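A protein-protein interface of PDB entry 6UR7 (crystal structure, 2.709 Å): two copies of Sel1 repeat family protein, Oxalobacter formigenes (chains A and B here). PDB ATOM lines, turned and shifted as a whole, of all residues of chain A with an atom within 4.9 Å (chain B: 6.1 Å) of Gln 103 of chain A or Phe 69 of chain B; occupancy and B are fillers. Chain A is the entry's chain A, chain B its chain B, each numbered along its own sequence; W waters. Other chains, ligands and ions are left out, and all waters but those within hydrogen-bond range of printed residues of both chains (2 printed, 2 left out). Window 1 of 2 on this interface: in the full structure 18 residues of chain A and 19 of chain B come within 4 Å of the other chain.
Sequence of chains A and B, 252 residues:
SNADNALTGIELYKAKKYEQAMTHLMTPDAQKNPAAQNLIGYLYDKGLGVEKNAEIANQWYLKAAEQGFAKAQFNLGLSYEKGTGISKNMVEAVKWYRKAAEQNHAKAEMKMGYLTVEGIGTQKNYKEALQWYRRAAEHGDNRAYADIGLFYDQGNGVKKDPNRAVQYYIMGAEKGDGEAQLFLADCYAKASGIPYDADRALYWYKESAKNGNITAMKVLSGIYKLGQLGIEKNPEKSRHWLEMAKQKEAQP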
ATOM      1  N   GLY A  68       3.941  10.896 -32.110  1.00  0.00           N
ATOM      2  CA  GLY A  68       3.043  10.799 -30.980  1.00  0.00           C
ATOM      3  C   GLY A  68       1.584  11.028 -31.295  1.00  0.00           C
ATOM      4  O   GLY A  68       0.785  11.187 -30.364  1.00  0.00           O
ATOM      5  N   ALA A  70      -1.885  10.121 -31.633  1.00  0.00           N
ATOM      6  CA  ALA A  70      -2.609   8.957 -31.131  1.00  0.00           C
ATOM      7  C   ALA A  70      -3.463   8.316 -32.217  1.00  0.00           C
ATOM      8  O   ALA A  70      -3.543   7.086 -32.310  1.00  0.00           O
ATOM      9  CB  ALA A  70      -3.476   9.353 -29.937  1.00  0.00           C
ATOM     10  N   GLN A  73      -1.087   6.000 -34.473  1.00  0.00           N
ATOM     11  CA  GLN A  73      -0.635   4.754 -33.867  1.00  0.00           C
ATOM     12  C   GLN A  73      -1.791   3.802 -33.588  1.00  0.00           C
ATOM     13  O   GLN A  73      -1.565   2.595 -33.446  1.00  0.00           O
ATOM     14  CB  GLN A  73       0.152   5.043 -32.588  1.00  0.00           C
ATOM     15  CG  GLN A  73      -0.427   6.134 -31.720  1.00  0.00           C
ATOM     16  CD  GLN A  73       0.598   6.716 -30.763  1.00  0.00           C
ATOM     17  OE1 GLN A  73       0.252   7.216 -29.692  1.00  0.00           O
ATOM     18  NE2 GLN A  73       1.866   6.662 -31.152  1.00  0.00           N
ATOM     19  N   LYS A  99       0.385   2.848 -26.983  1.00  0.00           N
ATOM     20  CA  LYS A  99       0.863   4.212 -27.194  1.00  0.00           C
ATOM     21  C   LYS A  99      -0.296   5.186 -27.361  1.00  0.00           C
ATOM     22  O   LYS A  99      -0.274   6.291 -26.807  1.00  0.00           O
ATOM     23  CB  LYS A  99       1.782   4.265 -28.415  1.00  0.00           C
ATOM     24  CG  LYS A  99       3.141   3.621 -28.211  1.00  0.00           C
ATOM     25  CD  LYS A  99       4.026   4.470 -27.314  1.00  0.00           C
ATOM     26  CE  LYS A  99       5.436   3.906 -27.239  1.00  0.00           C
ATOM     27  NZ  LYS A  99       6.332   4.761 -26.413  1.00  0.00           N
ATOM     28  N   ALA A 100      -1.323   4.792 -28.117  1.00  0.00           N
ATOM     29  CA  ALA A 100      -2.478   5.661 -28.308  1.00  0.00           C
ATOM     30  C   ALA A 100      -3.370   5.690 -27.073  1.00  0.00           C
ATOM     31  O   ALA A 100      -3.910   6.745 -26.721  1.00  0.00           O
ATOM     32  CB  ALA A 100      -3.277   5.213 -29.532  1.00  0.00           C
ATOM     33  N   ALA A 101      -3.531   4.547 -26.401  1.00  0.00           N
ATOM     34  CA  ALA A 101      -4.388   4.493 -25.221  1.00  0.00           C
ATOM     35  C   ALA A 101      -3.837   5.343 -24.083  1.00  0.00           C
ATOM     36  O   ALA A 101      -4.612   5.919 -23.311  1.00  0.00           O
ATOM     37  CB  ALA A 101      -4.567   3.046 -24.767  1.00  0.00           C
ATOM     38  N   GLU A 102      -2.510   5.435 -23.965  1.00  0.00           N
ATOM     39  CA  GLU A 102      -1.907   6.291 -22.950  1.00  0.00           C
ATOM     40  C   GLU A 102      -2.199   7.766 -23.189  1.00  0.00           C
ATOM     41  O   GLU A 102      -2.007   8.577 -22.277  1.00  0.00           O
ATOM     42  CB  GLU A 102      -0.395   6.062 -22.900  1.00  0.00           C
ATOM     43  CG  GLU A 102       0.008   4.695 -22.373  1.00  0.00           C
ATOM     44  CD  GLU A 102       1.502   4.449 -22.465  1.00  0.00           C
ATOM     45  OE1 GLU A 102       2.200   5.241 -23.133  1.00  0.00           O
ATOM     46  OE2 GLU A 102       1.980   3.459 -21.869  1.00  0.00           O
ATOM     47  N   GLN A 103      -2.658   8.131 -24.386  1.00  0.00           N
ATOM     48  CA  GLN A 103      -3.010   9.506 -24.714  1.00  0.00           C
ATOM     49  C   GLN A 103      -4.523   9.702 -24.787  1.00  0.00           C
ATOM     50  O   GLN A 103      -5.008  10.560 -25.529  1.00  0.00           O
ATOM     51  CB  GLN A 103      -2.349   9.930 -26.023  1.00  0.00           C
ATOM     52  CG  GLN A 103      -0.843   9.731 -26.042  1.00  0.00           C
ATOM     53  CD  GLN A 103      -0.193  10.293 -27.291  1.00  0.00           C
ATOM     54  OE1 GLN A 103      -0.617  11.320 -27.820  1.00  0.00           O
ATOM     55  NE2 GLN A 103       0.844   9.617 -27.771  1.00  0.00           N
ATOM     56  N   ASN A 104      -5.274   8.895 -24.032  1.00  0.00           N
ATOM     57  CA  ASN A 104      -6.723   9.035 -23.884  1.00  0.00           C
ATOM     58  C   ASN A 104      -7.474   8.770 -25.187  1.00  0.00           C
ATOM     59  O   ASN A 104      -8.505   9.394 -25.453  1.00  0.00           O
ATOM     60  CB  ASN A 104      -7.093  10.415 -23.329  1.00  0.00           C
ATOM     61  CG  ASN A 104      -6.339  10.752 -22.060  1.00  0.00           C
ATOM     62  OD1 ASN A 104      -5.993   9.868 -21.277  1.00  0.00           O
ATOM     63  ND2 ASN A 104      -6.076  12.037 -21.850  1.00  0.00           N
ATOM     64  N   HIS A 105      -6.982   7.843 -26.005  1.00  0.00           N
ATOM     65  CA  HIS A 105      -7.683   7.444 -27.221  1.00  0.00           C
ATOM     66  C   HIS A 105      -8.725   6.388 -26.870  1.00  0.00           C
ATOM     67  O   HIS A 105      -8.380   5.309 -26.374  1.00  0.00           O
ATOM     68  CB  HIS A 105      -6.693   6.914 -28.256  1.00  0.00           C
ATOM     69  CG  HIS A 105      -7.278   6.745 -29.623  1.00  0.00           C
ATOM     70  ND1 HIS A 105      -7.961   5.611 -30.008  1.00  0.00           N
ATOM     71  CD2 HIS A 105      -7.279   7.566 -30.700  1.00  0.00           C
ATOM     72  CE1 HIS A 105      -8.358   5.742 -31.261  1.00  0.00           C
ATOM     73  NE2 HIS A 105      -7.956   6.919 -31.705  1.00  0.00           N
ATOM     74  N   ASN B  33       5.057   6.847 -18.887  1.00  0.00           N
ATOM     75  CA  ASN B  33       3.760   7.155 -19.479  1.00  0.00           C
ATOM     76  C   ASN B  33       3.666   8.650 -19.766  1.00  0.00           C
ATOM     77  O   ASN B  33       3.890   9.463 -18.864  1.00  0.00           O
ATOM     78  CB  ASN B  33       2.641   6.725 -18.529  1.00  0.00           C
ATOM     79  CG  ASN B  33       1.262   6.828 -19.153  1.00  0.00           C
ATOM     80  OD1 ASN B  33       0.782   7.919 -19.460  1.00  0.00           O
ATOM     81  ND2 ASN B  33       0.604   5.687 -19.319  1.00  0.00           N
ATOM     82  N   PRO B  34       3.337   9.052 -20.998  1.00  0.00           N
ATOM     83  CA  PRO B  34       3.237  10.493 -21.284  1.00  0.00           C
ATOM     84  C   PRO B  34       2.142  11.188 -20.494  1.00  0.00           C
ATOM     85  O   PRO B  34       2.343  12.317 -20.029  1.00  0.00           O
ATOM     86  CB  PRO B  34       2.968  10.530 -22.795  1.00  0.00           C
ATOM     87  CG  PRO B  34       2.374   9.197 -23.110  1.00  0.00           C
ATOM     88  CD  PRO B  34       3.042   8.227 -22.181  1.00  0.00           C
ATOM     89  N   ALA B  35       0.984  10.544 -20.325  1.00  0.00           N
ATOM     90  CA  ALA B  35      -0.082  11.153 -19.536  1.00  0.00           C
ATOM     91  C   ALA B  35       0.322  11.281 -18.074  1.00  0.00           C
ATOM     92  O   ALA B  35      -0.028  12.265 -17.411  1.00  0.00           O
ATOM     93  CB  ALA B  35      -1.370  10.339 -19.669  1.00  0.00           C
ATOM     94  N   ALA B  36       1.061  10.299 -17.553  1.00  0.00           N
ATOM     95  CA  ALA B  36       1.558  10.394 -16.185  1.00  0.00           C
ATOM     96  C   ALA B  36       2.593  11.502 -16.051  1.00  0.00           C
ATOM     97  O   ALA B  36       2.605  12.229 -15.053  1.00  0.00           O
ATOM     98  CB  ALA B  36       2.143   9.053 -15.741  1.00  0.00           C
ATOM     99  N   ASN B  38       2.756  14.271 -17.799  1.00  0.00           N
ATOM    100  CA  ASN B  38       2.040  15.541 -17.787  1.00  0.00           C
ATOM    101  C   ASN B  38       1.342  15.766 -16.453  1.00  0.00           C
ATOM    102  O   ASN B  38       1.290  16.896 -15.955  1.00  0.00           O
ATOM    103  CB  ASN B  38       1.034  15.590 -18.937  1.00  0.00           C
ATOM    104  CG  ASN B  38       0.223  16.868 -18.944  1.00  0.00           C
ATOM    105  OD1 ASN B  38       0.729  17.936 -19.290  1.00  0.00           O
ATOM    106  ND2 ASN B  38      -1.046  16.767 -18.564  1.00  0.00           N
ATOM    107  N   LEU B  39       0.803  14.698 -15.860  1.00  0.00           N
ATOM    108  CA  LEU B  39       0.157  14.827 -14.558  1.00  0.00           C
ATOM    109  C   LEU B  39       1.169  15.135 -13.462  1.00  0.00           C
ATOM    110  O   LEU B  39       0.855  15.872 -12.520  1.00  0.00           O
ATOM    111  CB  LEU B  39      -0.620  13.550 -14.236  1.00  0.00           C
ATOM    112  CG  LEU B  39      -1.507  13.564 -12.989  1.00  0.00           C
ATOM    113  CD1 LEU B  39      -2.461  14.747 -13.022  1.00  0.00           C
ATOM    114  CD2 LEU B  39      -2.276  12.259 -12.875  1.00  0.00           C
ATOM    115  N   ALA B  64       6.823  14.656 -21.745  1.00  0.00           N
ATOM    116  CA  ALA B  64       5.579  14.192 -22.344  1.00  0.00           C
ATOM    117  C   ALA B  64       5.284  14.895 -23.663  1.00  0.00           C
ATOM    118  O   ALA B  64       4.702  14.284 -24.567  1.00  0.00           O
ATOM    119  CB  ALA B  64       4.420  14.387 -21.365  1.00  0.00           C
ATOM    120  N   ALA B  65       5.673  16.166 -23.796  1.00  0.00           N
ATOM    121  CA  ALA B  65       5.505  16.855 -25.071  1.00  0.00           C
ATOM    122  C   ALA B  65       6.386  16.250 -26.154  1.00  0.00           C
ATOM    123  O   ALA B  65       6.008  16.250 -27.332  1.00  0.00           O
ATOM    124  CB  ALA B  65       5.806  18.346 -24.914  1.00  0.00           C
ATOM    125  N   GLU B  66       7.560  15.734 -25.782  1.00  0.00           N
ATOM    126  CA  GLU B  66       8.416  15.057 -26.747  1.00  0.00           C
ATOM    127  C   GLU B  66       7.853  13.707 -27.171  1.00  0.00           C
ATOM    128  O   GLU B  66       8.266  13.175 -28.206  1.00  0.00           O
ATOM    129  CB  GLU B  66       9.823  14.879 -26.175  1.00  0.00           C
ATOM    130  CG  GLU B  66      10.636  16.160 -26.132  1.00  0.00           C
ATOM    131  CD  GLU B  66      12.011  15.957 -25.529  1.00  0.00           C
ATOM    132  OE1 GLU B  66      12.258  14.874 -24.960  1.00  0.00           O
ATOM    133  OE2 GLU B  66      12.845  16.881 -25.627  1.00  0.00           O
ATOM    134  N   GLN B  67       6.929  13.142 -26.397  1.00  0.00           N
ATOM    135  CA  GLN B  67       6.216  11.937 -26.798  1.00  0.00           C
ATOM    136  C   GLN B  67       4.983  12.238 -27.639  1.00  0.00           C
ATOM    137  O   GLN B  67       4.304  11.301 -28.073  1.00  0.00           O
ATOM    138  CB  GLN B  67       5.806  11.124 -25.565  1.00  0.00           C
ATOM    139  CG  GLN B  67       6.968  10.581 -24.753  1.00  0.00           C
ATOM    140  CD  GLN B  67       6.541   9.484 -23.798  1.00  0.00           C
ATOM    141  OE1 GLN B  67       6.199   8.377 -24.218  1.00  0.00           O
ATOM    142  NE2 GLN B  67       6.552   9.786 -22.503  1.00  0.00           N
ATOM    143  N   GLY B  68       4.676  13.511 -27.870  1.00  0.00           N
ATOM    144  CA  GLY B  68       3.529  13.893 -28.664  1.00  0.00           C
ATOM    145  C   GLY B  68       2.243  14.096 -27.896  1.00  0.00           C
ATOM    146  O   GLY B  68       1.175  14.154 -28.516  1.00  0.00           O
ATOM    147  N   PHE B  69       2.305  14.204 -26.571  1.00  0.00           N
ATOM    148  CA  PHE B  69       1.106  14.383 -25.762  1.00  0.00           C
ATOM    149  C   PHE B  69       0.633  15.828 -25.874  1.00  0.00           C
ATOM    150  O   PHE B  69       1.349  16.755 -25.477  1.00  0.00           O
ATOM    151  CB  PHE B  69       1.388  14.005 -24.310  1.00  0.00           C
ATOM    152  CG  PHE B  69       0.151  13.785 -23.488  1.00  0.00           C
ATOM    153  CD1 PHE B  69      -0.822  12.893 -23.903  1.00  0.00           C
ATOM    154  CD2 PHE B  69      -0.030  14.458 -22.291  1.00  0.00           C
ATOM    155  CE1 PHE B  69      -1.959  12.686 -23.149  1.00  0.00           C
ATOM    156  CE2 PHE B  69      -1.164  14.252 -21.530  1.00  0.00           C
ATOM    157  CZ  PHE B  69      -2.131  13.366 -21.960  1.00  0.00           C
ATOM    158  N   ALA B  70      -0.576  16.017 -26.411  1.00  0.00           N
ATOM    159  CA  ALA B  70      -1.055  17.363 -26.716  1.00  0.00           C
ATOM    160  C   ALA B  70      -1.224  18.203 -25.455  1.00  0.00           C
ATOM    161  O   ALA B  70      -0.944  19.408 -25.464  1.00  0.00           O
ATOM    162  CB  ALA B  70      -2.370  17.289 -27.491  1.00  0.00           C
ATOM    163  N   LYS B  71      -1.688  17.590 -24.361  1.00  0.00           N
ATOM    164  CA  LYS B  71      -1.848  18.334 -23.114  1.00  0.00           C
ATOM    165  C   LYS B  71      -0.519  18.906 -22.640  1.00  0.00           C
ATOM    166  O   LYS B  71      -0.448  20.063 -22.211  1.00  0.00           O
ATOM    167  CB  LYS B  71      -2.450  17.440 -22.031  1.00  0.00           C
ATOM    168  CG  LYS B  71      -3.922  17.112 -22.207  1.00  0.00           C
ATOM    169  CD  LYS B  71      -4.434  16.345 -20.996  1.00  0.00           C
ATOM    170  CE  LYS B  71      -5.902  15.989 -21.131  1.00  0.00           C
ATOM    171  NZ  LYS B  71      -6.399  15.273 -19.922  1.00  0.00           N
ATOM    172  N   ALA B  72       0.549  18.107 -22.707  1.00  0.00           N
ATOM    173  CA  ALA B  72       1.857  18.586 -22.278  1.00  0.00           C
ATOM    174  C   ALA B  72       2.389  19.657 -23.221  1.00  0.00           C
ATOM    175  O   ALA B  72       3.038  20.612 -22.780  1.00  0.00           O
ATOM    176  CB  ALA B  72       2.838  17.421 -22.183  1.00  0.00           C
ATOM    177  N   GLN B  73       2.129  19.513 -24.522  1.00  0.00           N
ATOM    178  CA  GLN B  73       2.516  20.553 -25.467  1.00  0.00           C
ATOM    179  C   GLN B  73       1.780  21.856 -25.188  1.00  0.00           C
ATOM    180  O   GLN B  73       2.343  22.940 -25.375  1.00  0.00           O
ATOM    181  CB  GLN B  73       2.258  20.080 -26.899  1.00  0.00           C
ATOM    182  CG  GLN B  73       3.104  18.880 -27.303  1.00  0.00           C
ATOM    183  CD  GLN B  73       2.661  18.259 -28.611  1.00  0.00           C
ATOM    184  OE1 GLN B  73       1.624  18.621 -29.164  1.00  0.00           O
ATOM    185  NE2 GLN B  73       3.447  17.314 -29.113  1.00  0.00           N
ATOM    186  N   PHE B  74       0.532  21.772 -24.723  1.00  0.00           N
ATOM    187  CA  PHE B  74      -0.207  22.978 -24.365  1.00  0.00           C
ATOM    188  C   PHE B  74       0.341  23.599 -23.086  1.00  0.00           C
ATOM    189  O   PHE B  74       0.570  24.812 -23.022  1.00  0.00           O
ATOM    190  CB  PHE B  74      -1.694  22.655 -24.215  1.00  0.00           C
ATOM    191  CG  PHE B  74      -2.509  23.795 -23.678  1.00  0.00           C
ATOM    192  CD1 PHE B  74      -2.905  24.832 -24.505  1.00  0.00           C
ATOM    193  CD2 PHE B  74      -2.885  23.827 -22.344  1.00  0.00           C
ATOM    194  CE1 PHE B  74      -3.656  25.883 -24.014  1.00  0.00           C
ATOM    195  CE2 PHE B  74      -3.637  24.875 -21.846  1.00  0.00           C
ATOM    196  CZ  PHE B  74      -4.022  25.904 -22.682  1.00  0.00           C
ATOM    197  N   ALA B 100       0.062  21.125 -30.321  1.00  0.00           N
ATOM    198  CA  ALA B 100      -1.125  20.623 -29.640  1.00  0.00           C
ATOM    199  C   ALA B 100      -2.389  20.891 -30.446  1.00  0.00           C
ATOM    200  O   ALA B 100      -3.261  20.020 -30.545  1.00  0.00           O
ATOM    201  CB  ALA B 100      -1.233  21.246 -28.249  1.00  0.00           C
ATOM    202  N   GLN B 103      -3.292  18.458 -33.025  1.00  0.00           N
ATOM    203  CA  GLN B 103      -3.832  17.208 -32.503  1.00  0.00           C
ATOM    204  C   GLN B 103      -5.211  17.393 -31.878  1.00  0.00           C
ATOM    205  O   GLN B 103      -5.569  16.676 -30.937  1.00  0.00           O
ATOM    206  CB  GLN B 103      -2.860  16.593 -31.497  1.00  0.00           C
ATOM    207  CG  GLN B 103      -1.520  16.201 -32.107  1.00  0.00           C
ATOM    208  CD  GLN B 103      -0.523  15.707 -31.076  1.00  0.00           C
ATOM    209  OE1 GLN B 103      -0.205  14.519 -31.021  1.00  0.00           O
ATOM    210  NE2 GLN B 103      -0.016  16.622 -30.257  1.00  0.00           N
HETATM  211  O   HOH W   1      -8.740  13.671 -21.897  1.00  0.00           O
HETATM  212  O   HOH W   2      -4.587  12.830 -19.164  1.00  0.00           O
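The backbone carbonyl oxygen (O) of Gly 68 of chain B lies close to the side-chain amide oxygen (OE1) of Gln 103 of chain A.
The backbone carbonyl oxygen of Ala 64 of chain B is in hydrogen-bond range of the backbone NH of Phe 69 of chain B (3.1 Å). The side-chain amide oxygen (OE1) of Gln 73 of chain B lies within hydrogen-bond range of the side-chain amide nitrogen (NE2) of Gln 103 of chain B (2.8 Å). O of Gly 68 of chain A lies close to OE1 of Gln 103 of chain A. OE1 of Gln 73 of chain A is in hydrogen-bond range of NE2 of Gln 103 of chain A (3.1 Å). OD1 of Asn 33 of chain B sits at hydrogen-bond distance from N of Ala 35 of chain B (2.8 Å). The backbone carbonyl oxygen (O) of Gly 68 of chain B sits close to the side-chain amide oxygen (OE1) of Gln 103 of chain B.
Among the printed residues, merely in contact across the chains: Gly 68 of chain A with Gln 67 of chain B (3.2 Å), Gly 68 of chain A with Gly 68 of chain B (3.5 Å), Gly 68 of chain A with Gln 103 of chain B (3.5 Å), Glu 102 of chain A with Asn 33 of chain B (3.3 Å), Glu 102 of chain A with Pro 34 of chain B (3.2 Å), Glu 102 of chain A with Ala 35 of chain B (3.2 Å), Gln 103 of chain A with Gln 67 of chain B (3.9 Å), Gln 103 of chain A with Phe 69 of chain B (3.7 Å) and Asn 104 of chain A with Lys 71 of chain B (3.8 Å).
Of chain B, only Gln 67 (3.9 Å), Gly 68 (3.4 Å) and Phe 69 (3.7 Å) come within 4 Å of Gln 103 of chain A. Of the printed residues of chain A, Phe 69 of chain B touches Gln 103. Of the printed residues of chain A, Pro 34 of chain B touches Glu 102 (3.2 Å). Printed residues of chain B within 4 Å of Gly 68 of chain A: Gln 67, Gly 68 and Gln 103. Of the printed residues of chain A, Gly 68 of chain B touches Gly 68 and Gln 103. Of the printed residues of chain A, Gln 67 of chain B touches Gly 68 and Gln 103. Printed residues of chain A within 4 Å of Ala 35 of chain B: Glu 102. Lys 99 of chain A touches none of the printed residues of chain B. Ala 36 of chain B touches none of the printed residues of chain A. The nearest residue of chain A that does not touch Phe 69 of chain B is Asn 104 of chain A (4.2 Å). The nearest printed residue of chain A that does not touch Asn 33 of chain B is Gln 103 of chain A (6.0 Å).
Of the 19 printed residues of chain B, 8 touch a printed residue of chain A. Hydrophobic or aromatic side chains of chain B within 4 Å of the printed part of chain A: Pro 34, Ala 35 and Phe 69. Of the 10 printed residues of chain A, 4 touch a printed residue of chain B. Along chain A the printed residues that touch a printed residue of chain B span positions 68 to 104. Among the printed residues, 10 pairs touch across the chains.
Gly 68 of chain A touches its own counterpart, Gly 68 of chain B. Gly 68 of chain A touches Gln 103 of chain B, and with the chains exchanged Gln 103 of chain A touches Gly 68 of chain B. 5 positions are printed for both chains.
Water W1 lies within hydrogen-bond range of ND2 of Asn 104 of chain A (3.1 Å) and NZ of Lys 71 of chain B (3.5 Å). Water W2 bridges the side-chain amino group of Lys 71 of chain B (3.1 Å) and the side-chain amide nitrogen of Asn 104 of chain A (3.2 Å).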
